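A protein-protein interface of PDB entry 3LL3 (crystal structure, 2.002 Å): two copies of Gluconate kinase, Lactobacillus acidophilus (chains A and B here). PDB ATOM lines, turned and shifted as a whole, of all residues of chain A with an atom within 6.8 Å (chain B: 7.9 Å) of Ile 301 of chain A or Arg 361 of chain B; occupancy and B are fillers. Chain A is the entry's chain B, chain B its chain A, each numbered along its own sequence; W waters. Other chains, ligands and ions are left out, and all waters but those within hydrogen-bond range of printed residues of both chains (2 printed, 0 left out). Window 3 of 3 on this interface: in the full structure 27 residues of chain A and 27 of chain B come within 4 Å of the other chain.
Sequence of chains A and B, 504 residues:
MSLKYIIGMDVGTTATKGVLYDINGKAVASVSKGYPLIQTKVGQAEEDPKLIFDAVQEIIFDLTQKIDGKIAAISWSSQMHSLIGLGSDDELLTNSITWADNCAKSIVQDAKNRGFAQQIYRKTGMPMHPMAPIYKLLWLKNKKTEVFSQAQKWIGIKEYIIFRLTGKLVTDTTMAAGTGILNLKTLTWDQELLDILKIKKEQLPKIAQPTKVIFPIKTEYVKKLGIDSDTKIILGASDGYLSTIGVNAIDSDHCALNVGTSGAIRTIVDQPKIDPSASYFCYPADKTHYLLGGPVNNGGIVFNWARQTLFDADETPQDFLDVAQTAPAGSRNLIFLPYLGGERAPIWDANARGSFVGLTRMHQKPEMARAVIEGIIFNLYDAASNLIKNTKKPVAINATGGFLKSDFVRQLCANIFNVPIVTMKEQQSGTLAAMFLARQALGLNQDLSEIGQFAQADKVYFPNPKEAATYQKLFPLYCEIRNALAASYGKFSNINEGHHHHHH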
ATOM      1  N   GLY A 260      14.310 -11.614  -8.561  1.00  0.00           N
ATOM      2  CA  GLY A 260      14.729 -12.654  -9.486  1.00  0.00           C
ATOM      3  C   GLY A 260      13.536 -13.135 -10.285  1.00  0.00           C
ATOM      4  O   GLY A 260      12.861 -12.338 -10.945  1.00  0.00           O
ATOM      5  N   THR A 261      13.276 -14.435 -10.237  1.00  0.00           N
ATOM      6  CA  THR A 261      12.054 -14.982 -10.818  1.00  0.00           C
ATOM      7  C   THR A 261      10.851 -14.334 -10.132  1.00  0.00           C
ATOM      8  O   THR A 261       9.915 -13.838 -10.781  1.00  0.00           O
ATOM      9  CB  THR A 261      11.988 -16.506 -10.634  1.00  0.00           C
ATOM     10  OG1 THR A 261      13.083 -17.112 -11.326  1.00  0.00           O
ATOM     11  CG2 THR A 261      10.708 -17.043 -11.212  1.00  0.00           C
ATOM     12  N   SER A 262      10.885 -14.334  -8.804  1.00  0.00           N
ATOM     13  CA  SER A 262       9.939 -13.554  -8.025  1.00  0.00           C
ATOM     14  C   SER A 262      10.700 -12.474  -7.260  1.00  0.00           C
ATOM     15  O   SER A 262      11.912 -12.327  -7.392  1.00  0.00           O
ATOM     16  CB  SER A 262       9.169 -14.447  -7.060  1.00  0.00           C
ATOM     17  OG  SER A 262      10.046 -15.012  -6.107  1.00  0.00           O
ATOM     18  N   ASN A 297       5.037 -12.204  -6.216  1.00  0.00           N
ATOM     19  CA  ASN A 297       5.171 -13.318  -7.162  1.00  0.00           C
ATOM     20  C   ASN A 297       5.749 -12.916  -8.517  1.00  0.00           C
ATOM     21  O   ASN A 297       6.606 -13.612  -9.080  1.00  0.00           O
ATOM     22  CB  ASN A 297       3.807 -13.952  -7.466  1.00  0.00           C
ATOM     23  CG  ASN A 297       3.157 -14.565  -6.258  1.00  0.00           C
ATOM     24  OD1 ASN A 297       3.806 -14.801  -5.254  1.00  0.00           O
ATOM     25  ND2 ASN A 297       1.854 -14.827  -6.357  1.00  0.00           N
ATOM     26  N   ASN A 298       5.225 -11.818  -9.055  1.00  0.00           N
ATOM     27  CA  ASN A 298       5.369 -11.495 -10.476  1.00  0.00           C
ATOM     28  C   ASN A 298       6.593 -10.656 -10.795  1.00  0.00           C
ATOM     29  O   ASN A 298       6.493  -9.472 -11.098  1.00  0.00           O
ATOM     30  CB  ASN A 298       4.071 -10.855 -10.985  1.00  0.00           C
ATOM     31  CG  ASN A 298       2.873 -11.792 -10.806  1.00  0.00           C
ATOM     32  OD1 ASN A 298       2.773 -12.815 -11.473  1.00  0.00           O
ATOM     33  ND2 ASN A 298       1.994 -11.468  -9.862  1.00  0.00           N
ATOM     34  N   GLY A 299       7.761 -11.294 -10.721  1.00  0.00           N
ATOM     35  CA  GLY A 299       9.021 -10.631 -11.003  1.00  0.00           C
ATOM     36  C   GLY A 299       9.552 -10.996 -12.387  1.00  0.00           C
ATOM     37  O   GLY A 299       8.869 -10.830 -13.384  1.00  0.00           O
ATOM     38  N   GLY A 300      10.774 -11.514 -12.435  1.00  0.00           N
ATOM     39  CA  GLY A 300      11.379 -11.944 -13.678  1.00  0.00           C
ATOM     40  C   GLY A 300      10.605 -13.034 -14.392  1.00  0.00           C
ATOM     41  O   GLY A 300      10.754 -13.208 -15.596  1.00  0.00           O
ATOM     42  N   ILE A 301       9.799 -13.787 -13.655  1.00  0.00           N
ATOM     43  CA  ILE A 301       8.974 -14.813 -14.281  1.00  0.00           C
ATOM     44  C   ILE A 301       8.026 -14.184 -15.319  1.00  0.00           C
ATOM     45  O   ILE A 301       7.783 -14.756 -16.378  1.00  0.00           O
ATOM     46  CB  ILE A 301       8.185 -15.631 -13.232  1.00  0.00           C
ATOM     47  CG1 ILE A 301       7.486 -16.821 -13.884  1.00  0.00           C
ATOM     48  CG2 ILE A 301       7.190 -14.762 -12.486  1.00  0.00           C
ATOM     49  CD1 ILE A 301       6.922 -17.828 -12.874  1.00  0.00           C
ATOM     50  N   VAL A 302       7.525 -12.988 -15.016  1.00  0.00           N
ATOM     51  CA  VAL A 302       6.623 -12.269 -15.912  1.00  0.00           C
ATOM     52  C   VAL A 302       7.409 -11.667 -17.080  1.00  0.00           C
ATOM     53  O   VAL A 302       6.963 -11.705 -18.222  1.00  0.00           O
ATOM     54  CB  VAL A 302       5.795 -11.214 -15.144  1.00  0.00           C
ATOM     55  CG1 VAL A 302       4.976 -10.339 -16.105  1.00  0.00           C
ATOM     56  CG2 VAL A 302       4.887 -11.918 -14.123  1.00  0.00           C
ATOM     57  N   PHE A 303       8.605 -11.157 -16.800  1.00  0.00           N
ATOM     58  CA  PHE A 303       9.504 -10.705 -17.853  1.00  0.00           C
ATOM     59  C   PHE A 303       9.756 -11.839 -18.847  1.00  0.00           C
ATOM     60  O   PHE A 303       9.723 -11.630 -20.057  1.00  0.00           O
ATOM     61  CB  PHE A 303      10.844 -10.254 -17.252  1.00  0.00           C
ATOM     62  CG  PHE A 303      11.854  -9.816 -18.278  1.00  0.00           C
ATOM     63  CD1 PHE A 303      12.767 -10.718 -18.802  1.00  0.00           C
ATOM     64  CD2 PHE A 303      11.873  -8.506 -18.736  1.00  0.00           C
ATOM     65  CE1 PHE A 303      13.695 -10.306 -19.760  1.00  0.00           C
ATOM     66  CE2 PHE A 303      12.798  -8.090 -19.678  1.00  0.00           C
ATOM     67  CZ  PHE A 303      13.713  -8.987 -20.185  1.00  0.00           C
ATOM     68  N   ASN A 304      10.028 -13.034 -18.321  1.00  0.00           N
ATOM     69  CA  ASN A 304      10.305 -14.196 -19.159  1.00  0.00           C
ATOM     70  C   ASN A 304       9.083 -14.583 -20.003  1.00  0.00           C
ATOM     71  O   ASN A 304       9.208 -14.877 -21.179  1.00  0.00           O
ATOM     72  CB  ASN A 304      10.799 -15.385 -18.318  1.00  0.00           C
ATOM     73  CG  ASN A 304      11.269 -16.544 -19.179  1.00  0.00           C
ATOM     74  OD1 ASN A 304      10.668 -17.628 -19.179  1.00  0.00           O
ATOM     75  ND2 ASN A 304      12.338 -16.322 -19.927  1.00  0.00           N
ATOM     76  N   TRP A 305       7.898 -14.542 -19.404  1.00  0.00           N
ATOM     77  CA  TRP A 305       6.661 -14.758 -20.150  1.00  0.00           C
ATOM     78  C   TRP A 305       6.544 -13.803 -21.340  1.00  0.00           C
ATOM     79  O   TRP A 305       6.294 -14.232 -22.476  1.00  0.00           O
ATOM     80  CB  TRP A 305       5.445 -14.580 -19.254  1.00  0.00           C
ATOM     81  CG  TRP A 305       4.188 -14.564 -20.040  1.00  0.00           C
ATOM     82  CD1 TRP A 305       3.520 -15.645 -20.533  1.00  0.00           C
ATOM     83  CD2 TRP A 305       3.446 -13.410 -20.453  1.00  0.00           C
ATOM     84  NE1 TRP A 305       2.396 -15.234 -21.218  1.00  0.00           N
ATOM     85  CE2 TRP A 305       2.333 -13.869 -21.190  1.00  0.00           C
ATOM     86  CE3 TRP A 305       3.609 -12.035 -20.264  1.00  0.00           C
ATOM     87  CZ2 TRP A 305       1.391 -13.000 -21.739  1.00  0.00           C
ATOM     88  CZ3 TRP A 305       2.681 -11.176 -20.810  1.00  0.00           C
ATOM     89  CH2 TRP A 305       1.580 -11.660 -21.543  1.00  0.00           C
ATOM     90  N   ALA A 306       6.734 -12.512 -21.077  1.00  0.00           N
ATOM     91  CA  ALA A 306       6.610 -11.484 -22.105  1.00  0.00           C
ATOM     92  C   ALA A 306       7.674 -11.637 -23.184  1.00  0.00           C
ATOM     93  O   ALA A 306       7.385 -11.495 -24.371  1.00  0.00           O
ATOM     94  CB  ALA A 306       6.662 -10.087 -21.488  1.00  0.00           C
ATOM     95  N   THR A 309       6.292 -14.448 -25.276  1.00  0.00           N
ATOM     96  CA  THR A 309       4.937 -14.311 -25.781  1.00  0.00           C
ATOM     97  C   THR A 309       4.820 -13.111 -26.710  1.00  0.00           C
ATOM     98  O   THR A 309       4.233 -13.196 -27.779  1.00  0.00           O
ATOM     99  CB  THR A 309       3.947 -14.149 -24.620  1.00  0.00           C
ATOM    100  OG1 THR A 309       3.903 -15.360 -23.872  1.00  0.00           O
ATOM    101  CG2 THR A 309       2.538 -13.805 -25.130  1.00  0.00           C
ATOM    102  N   LEU A 340       0.217 -12.073 -13.417  1.00  0.00           N
ATOM    103  CA  LEU A 340      -0.034 -13.298 -14.174  1.00  0.00           C
ATOM    104  C   LEU A 340      -0.259 -14.529 -13.308  1.00  0.00           C
ATOM    105  O   LEU A 340      -1.083 -15.370 -13.638  1.00  0.00           O
ATOM    106  CB  LEU A 340       1.093 -13.585 -15.170  1.00  0.00           C
ATOM    107  CG  LEU A 340       0.888 -12.916 -16.529  1.00  0.00           C
ATOM    108  CD1 LEU A 340       0.809 -11.432 -16.357  1.00  0.00           C
ATOM    109  CD2 LEU A 340       2.040 -13.297 -17.431  1.00  0.00           C
ATOM    110  N   GLY A 341       0.484 -14.662 -12.216  1.00  0.00           N
ATOM    111  CA  GLY A 341       0.373 -15.876 -11.408  1.00  0.00           C
ATOM    112  C   GLY A 341      -0.406 -15.686 -10.123  1.00  0.00           C
ATOM    113  O   GLY A 341      -0.076 -16.289  -9.110  1.00  0.00           O
ATOM    114  N   ILE A 376       5.978  -4.387 -13.916  1.00  0.00           N
ATOM    115  CA  ILE A 376       6.613  -5.227 -12.919  1.00  0.00           C
ATOM    116  C   ILE A 376       7.174  -4.315 -11.824  1.00  0.00           C
ATOM    117  O   ILE A 376       6.964  -4.541 -10.637  1.00  0.00           O
ATOM    118  CB  ILE A 376       7.712  -6.087 -13.540  1.00  0.00           C
ATOM    119  CG1 ILE A 376       7.088  -7.176 -14.414  1.00  0.00           C
ATOM    120  CG2 ILE A 376       8.611  -6.711 -12.432  1.00  0.00           C
ATOM    121  CD1 ILE A 376       8.069  -7.842 -15.371  1.00  0.00           C
ATOM    122  N   PHE A 403      16.555 -10.024 -12.346  1.00  0.00           N
ATOM    123  CA  PHE A 403      15.696  -9.074 -13.057  1.00  0.00           C
ATOM    124  C   PHE A 403      16.324  -7.687 -13.065  1.00  0.00           C
ATOM    125  O   PHE A 403      16.085  -6.897 -13.992  1.00  0.00           O
ATOM    126  CB  PHE A 403      14.283  -9.019 -12.479  1.00  0.00           C
ATOM    127  CG  PHE A 403      13.389  -8.025 -13.169  1.00  0.00           C
ATOM    128  CD1 PHE A 403      12.982  -8.227 -14.486  1.00  0.00           C
ATOM    129  CD2 PHE A 403      12.973  -6.875 -12.512  1.00  0.00           C
ATOM    130  CE1 PHE A 403      12.164  -7.311 -15.121  1.00  0.00           C
ATOM    131  CE2 PHE A 403      12.157  -5.951 -13.146  1.00  0.00           C
ATOM    132  CZ  PHE A 403      11.754  -6.162 -14.449  1.00  0.00           C
ATOM    133  N   ARG B 332      -8.935 -19.307 -23.678  1.00  0.00           N
ATOM    134  CA  ARG B 332      -8.735 -19.568 -22.253  1.00  0.00           C
ATOM    135  C   ARG B 332      -9.190 -18.392 -21.401  1.00  0.00           C
ATOM    136  O   ARG B 332      -8.550 -18.036 -20.401  1.00  0.00           O
ATOM    137  CB  ARG B 332      -7.270 -19.897 -21.968  1.00  0.00           C
ATOM    138  CG  ARG B 332      -6.716 -21.017 -22.838  1.00  0.00           C
ATOM    139  CD  ARG B 332      -5.329 -21.432 -22.368  1.00  0.00           C
ATOM    140  NE  ARG B 332      -4.679 -22.271 -23.361  1.00  0.00           N
ATOM    141  CZ  ARG B 332      -4.783 -23.595 -23.383  1.00  0.00           C
ATOM    142  NH1 ARG B 332      -5.499 -24.218 -22.446  1.00  0.00           N
ATOM    143  NH2 ARG B 332      -4.170 -24.295 -24.326  1.00  0.00           N
ATOM    144  N   GLY B 358      -7.126 -10.583 -18.265  1.00  0.00           N
ATOM    145  CA  GLY B 358      -7.235 -11.985 -17.896  1.00  0.00           C
ATOM    146  C   GLY B 358      -6.009 -12.828 -18.205  1.00  0.00           C
ATOM    147  O   GLY B 358      -6.108 -14.032 -18.364  1.00  0.00           O
ATOM    148  N   LEU B 359      -4.849 -12.194 -18.302  1.00  0.00           N
ATOM    149  CA  LEU B 359      -3.634 -12.895 -18.695  1.00  0.00           C
ATOM    150  C   LEU B 359      -3.051 -13.765 -17.566  1.00  0.00           C
ATOM    151  O   LEU B 359      -3.163 -13.453 -16.377  1.00  0.00           O
ATOM    152  CB  LEU B 359      -2.564 -11.917 -19.179  1.00  0.00           C
ATOM    153  CG  LEU B 359      -2.738 -11.142 -20.485  1.00  0.00           C
ATOM    154  CD1 LEU B 359      -1.797  -9.947 -20.493  1.00  0.00           C
ATOM    155  CD2 LEU B 359      -2.475 -12.047 -21.695  1.00  0.00           C
ATOM    156  N   THR B 360      -2.424 -14.856 -17.982  1.00  0.00           N
ATOM    157  CA  THR B 360      -1.805 -15.820 -17.104  1.00  0.00           C
ATOM    158  C   THR B 360      -0.696 -16.400 -17.957  1.00  0.00           C
ATOM    159  O   THR B 360      -0.659 -16.154 -19.154  1.00  0.00           O
ATOM    160  CB  THR B 360      -2.833 -16.895 -16.751  1.00  0.00           C
ATOM    161  OG1 THR B 360      -2.708 -17.262 -15.381  1.00  0.00           O
ATOM    162  CG2 THR B 360      -2.665 -18.107 -17.622  1.00  0.00           C
ATOM    163  N   ARG B 361       0.209 -17.174 -17.373  1.00  0.00           N
ATOM    164  CA  ARG B 361       1.309 -17.730 -18.151  1.00  0.00           C
ATOM    165  C   ARG B 361       0.817 -18.796 -19.151  1.00  0.00           C
ATOM    166  O   ARG B 361       1.550 -19.208 -20.033  1.00  0.00           O
ATOM    167  CB  ARG B 361       2.425 -18.251 -17.213  1.00  0.00           C
ATOM    168  CG  ARG B 361       3.125 -17.105 -16.418  1.00  0.00           C
ATOM    169  CD  ARG B 361       3.866 -17.572 -15.141  1.00  0.00           C
ATOM    170  NE  ARG B 361       4.700 -18.748 -15.364  1.00  0.00           N
ATOM    171  CZ  ARG B 361       4.607 -19.876 -14.670  1.00  0.00           C
ATOM    172  NH1 ARG B 361       3.725 -19.978 -13.679  1.00  0.00           N
ATOM    173  NH2 ARG B 361       5.412 -20.898 -14.954  1.00  0.00           N
ATOM    174  N   MET B 362      -0.435 -19.223 -19.015  1.00  0.00           N
ATOM    175  CA  MET B 362      -1.073 -20.099 -20.013  1.00  0.00           C
ATOM    176  C   MET B 362      -1.381 -19.369 -21.328  1.00  0.00           C
ATOM    177  O   MET B 362      -1.561 -20.003 -22.364  1.00  0.00           O
ATOM    178  CB  MET B 362      -2.389 -20.685 -19.483  1.00  0.00           C
ATOM    179  CG  MET B 362      -2.234 -21.596 -18.288  1.00  0.00           C
ATOM    180  SD  MET B 362      -1.171 -23.158 -18.766  1.00  0.00           S
ATOM    181  CE  MET B 362      -2.454 -24.034 -19.969  1.00  0.00           C
ATOM    182  N   HIS B 363      -1.466 -18.045 -21.283  1.00  0.00           N
ATOM    183  CA  HIS B 363      -1.766 -17.274 -22.488  1.00  0.00           C
ATOM    184  C   HIS B 363      -0.520 -16.938 -23.278  1.00  0.00           C
ATOM    185  O   HIS B 363       0.233 -16.030 -22.915  1.00  0.00           O
ATOM    186  CB  HIS B 363      -2.538 -16.007 -22.148  1.00  0.00           C
ATOM    187  CG  HIS B 363      -3.846 -16.276 -21.480  1.00  0.00           C
ATOM    188  ND1 HIS B 363      -4.006 -16.217 -20.114  1.00  0.00           N
ATOM    189  CD2 HIS B 363      -5.049 -16.638 -21.989  1.00  0.00           C
ATOM    190  CE1 HIS B 363      -5.253 -16.524 -19.807  1.00  0.00           C
ATOM    191  NE2 HIS B 363      -5.910 -16.782 -20.926  1.00  0.00           N
ATOM    192  N   GLN B 364      -0.317 -17.666 -24.372  1.00  0.00           N
ATOM    193  CA  GLN B 364       0.822 -17.441 -25.246  1.00  0.00           C
ATOM    194  C   GLN B 364       0.359 -16.669 -26.481  1.00  0.00           C
ATOM    195  O   GLN B 364      -0.766 -16.186 -26.502  1.00  0.00           O
ATOM    196  CB  GLN B 364       1.469 -18.778 -25.603  1.00  0.00           C
ATOM    197  CG  GLN B 364       2.032 -19.498 -24.378  1.00  0.00           C
ATOM    198  CD  GLN B 364       2.401 -20.938 -24.669  1.00  0.00           C
ATOM    199  OE1 GLN B 364       3.237 -21.214 -25.526  1.00  0.00           O
ATOM    200  NE2 GLN B 364       1.772 -21.868 -23.953  1.00  0.00           N
ATOM    201  N   GLU B 367      -3.235 -17.434 -27.960  1.00  0.00           N
ATOM    202  CA  GLU B 367      -4.315 -16.919 -27.122  1.00  0.00           C
ATOM    203  C   GLU B 367      -4.526 -15.408 -27.305  1.00  0.00           C
ATOM    204  O   GLU B 367      -5.661 -14.941 -27.317  1.00  0.00           O
ATOM    205  CB  GLU B 367      -4.045 -17.214 -25.642  1.00  0.00           C
ATOM    206  CG  GLU B 367      -4.345 -18.655 -25.196  1.00  0.00           C
ATOM    207  CD  GLU B 367      -3.380 -19.680 -25.778  1.00  0.00           C
ATOM    208  OE1 GLU B 367      -2.206 -19.347 -26.065  1.00  0.00           O
ATOM    209  OE2 GLU B 367      -3.807 -20.829 -25.948  1.00  0.00           O
HETATM  210  O   HOH W   1       0.396 -17.893 -14.605  1.00  0.00           O
HETATM  211  O   HOH W   2      -2.762 -16.924 -12.043  1.00  0.00           O
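O of Leu 340 of chain A lies within hydrogen-bond range of OG1 of Thr 360 of chain B, at 3.0 Å.
The indole nitrogen (NE1) of Trp 305 of chain A lies within hydrogen-bond range of the backbone carbonyl oxygen (O) of His 363 of chain B, at 2.9 Å.
The backbone carbonyl oxygen (O) of Arg 332 of chain B is in hydrogen-bond range of a ring nitrogen (NE2) of His 363 of chain B, at 3.0 Å.
The backbone NH of Thr 360 of chain B sits at hydrogen-bond distance from a ring nitrogen (ND1) of His 363 of chain B (3.0 Å).
N of Leu 340 of chain A is in hydrogen-bond range of OD1 of Asn 298 of chain A (3.3 Å).
O of Thr 261 of chain A lies within hydrogen-bond range of N of Ile 301 of chain A, at 2.9 Å.
The backbone carbonyl oxygen (O) of Trp 305 of chain A sits at hydrogen-bond distance from the side-chain hydroxyl (OG1) of Thr 309 of chain A, 3.0 Å away.
The side-chain carboxylate of Glu 367 of chain B sits at hydrogen-bond distance from the backbone NH of Gln 364 of chain B (3.0 Å).
Among the printed residues, merely in contact across the chains: Ile 301 of chain A with Arg 361 of chain B (3.5 Å), Trp 305 of chain A with Leu 359 of chain B (3.9 Å), Trp 305 of chain A with Thr 360 of chain B (3.8 Å), Trp 305 of chain A with Arg 361 of chain B (3.9 Å), Thr 309 of chain A with His 363 of chain B (3.9 Å), Thr 309 of chain A with Gln 364 of chain B (3.8 Å) and Leu 340 of chain A with Leu 359 of chain B (3.8 Å).
Gly 300 of chain A touches none of the printed residues of chain B.
Of the printed residues of chain A, Thr 360 of chain B touches Trp 305 and Leu 340.
Printed residues of chain B within 4 Å of Leu 340 of chain A: Leu 359 (3.8 Å) and Thr 360 (3.0 Å).
Printed residues of chain B within 4 Å of Thr 309 of chain A: His 363 and Gln 364.
Of the printed residues of chain A, His 363 of chain B touches Trp 305 (2.9 Å) and Thr 309 (3.9 Å).
Gly 260 of chain A touches none of the printed residues of chain B.
Arg 332 of chain B touches none of the printed residues of chain A.
The nearest residue of chain A that does not touch Arg 361 of chain B is Leu 340 of chain A (4.1 Å).
Printed residues of chain A that touch a printed residue of chain B: Ile 301, Trp 305, Thr 309 and Leu 340.
Of the 9 printed residues of chain B, 5 touch a printed residue of chain A.
Along chain B the printed residues that touch a printed residue of chain A span positions 359 to 364.
Among the printed residues, 9 pairs touch across the chains.
No position is printed for both chains.
Of the 9 pairs that touch across the chains among the printed residues, none has its exchanged pair printed and touching as well.
Water W2 lies within hydrogen-bond range of the backbone carbonyl oxygen of Leu 340 of chain A (2.8 Å) and the side-chain hydroxyl of Thr 360 of chain B (3.4 Å).
Water W1 lies within hydrogen-bond range of N of Arg 361 of chain B (2.9 Å), O of Leu 340 of chain A (3.1 Å) and OG1 of Thr 360 of chain B (3.3 Å).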
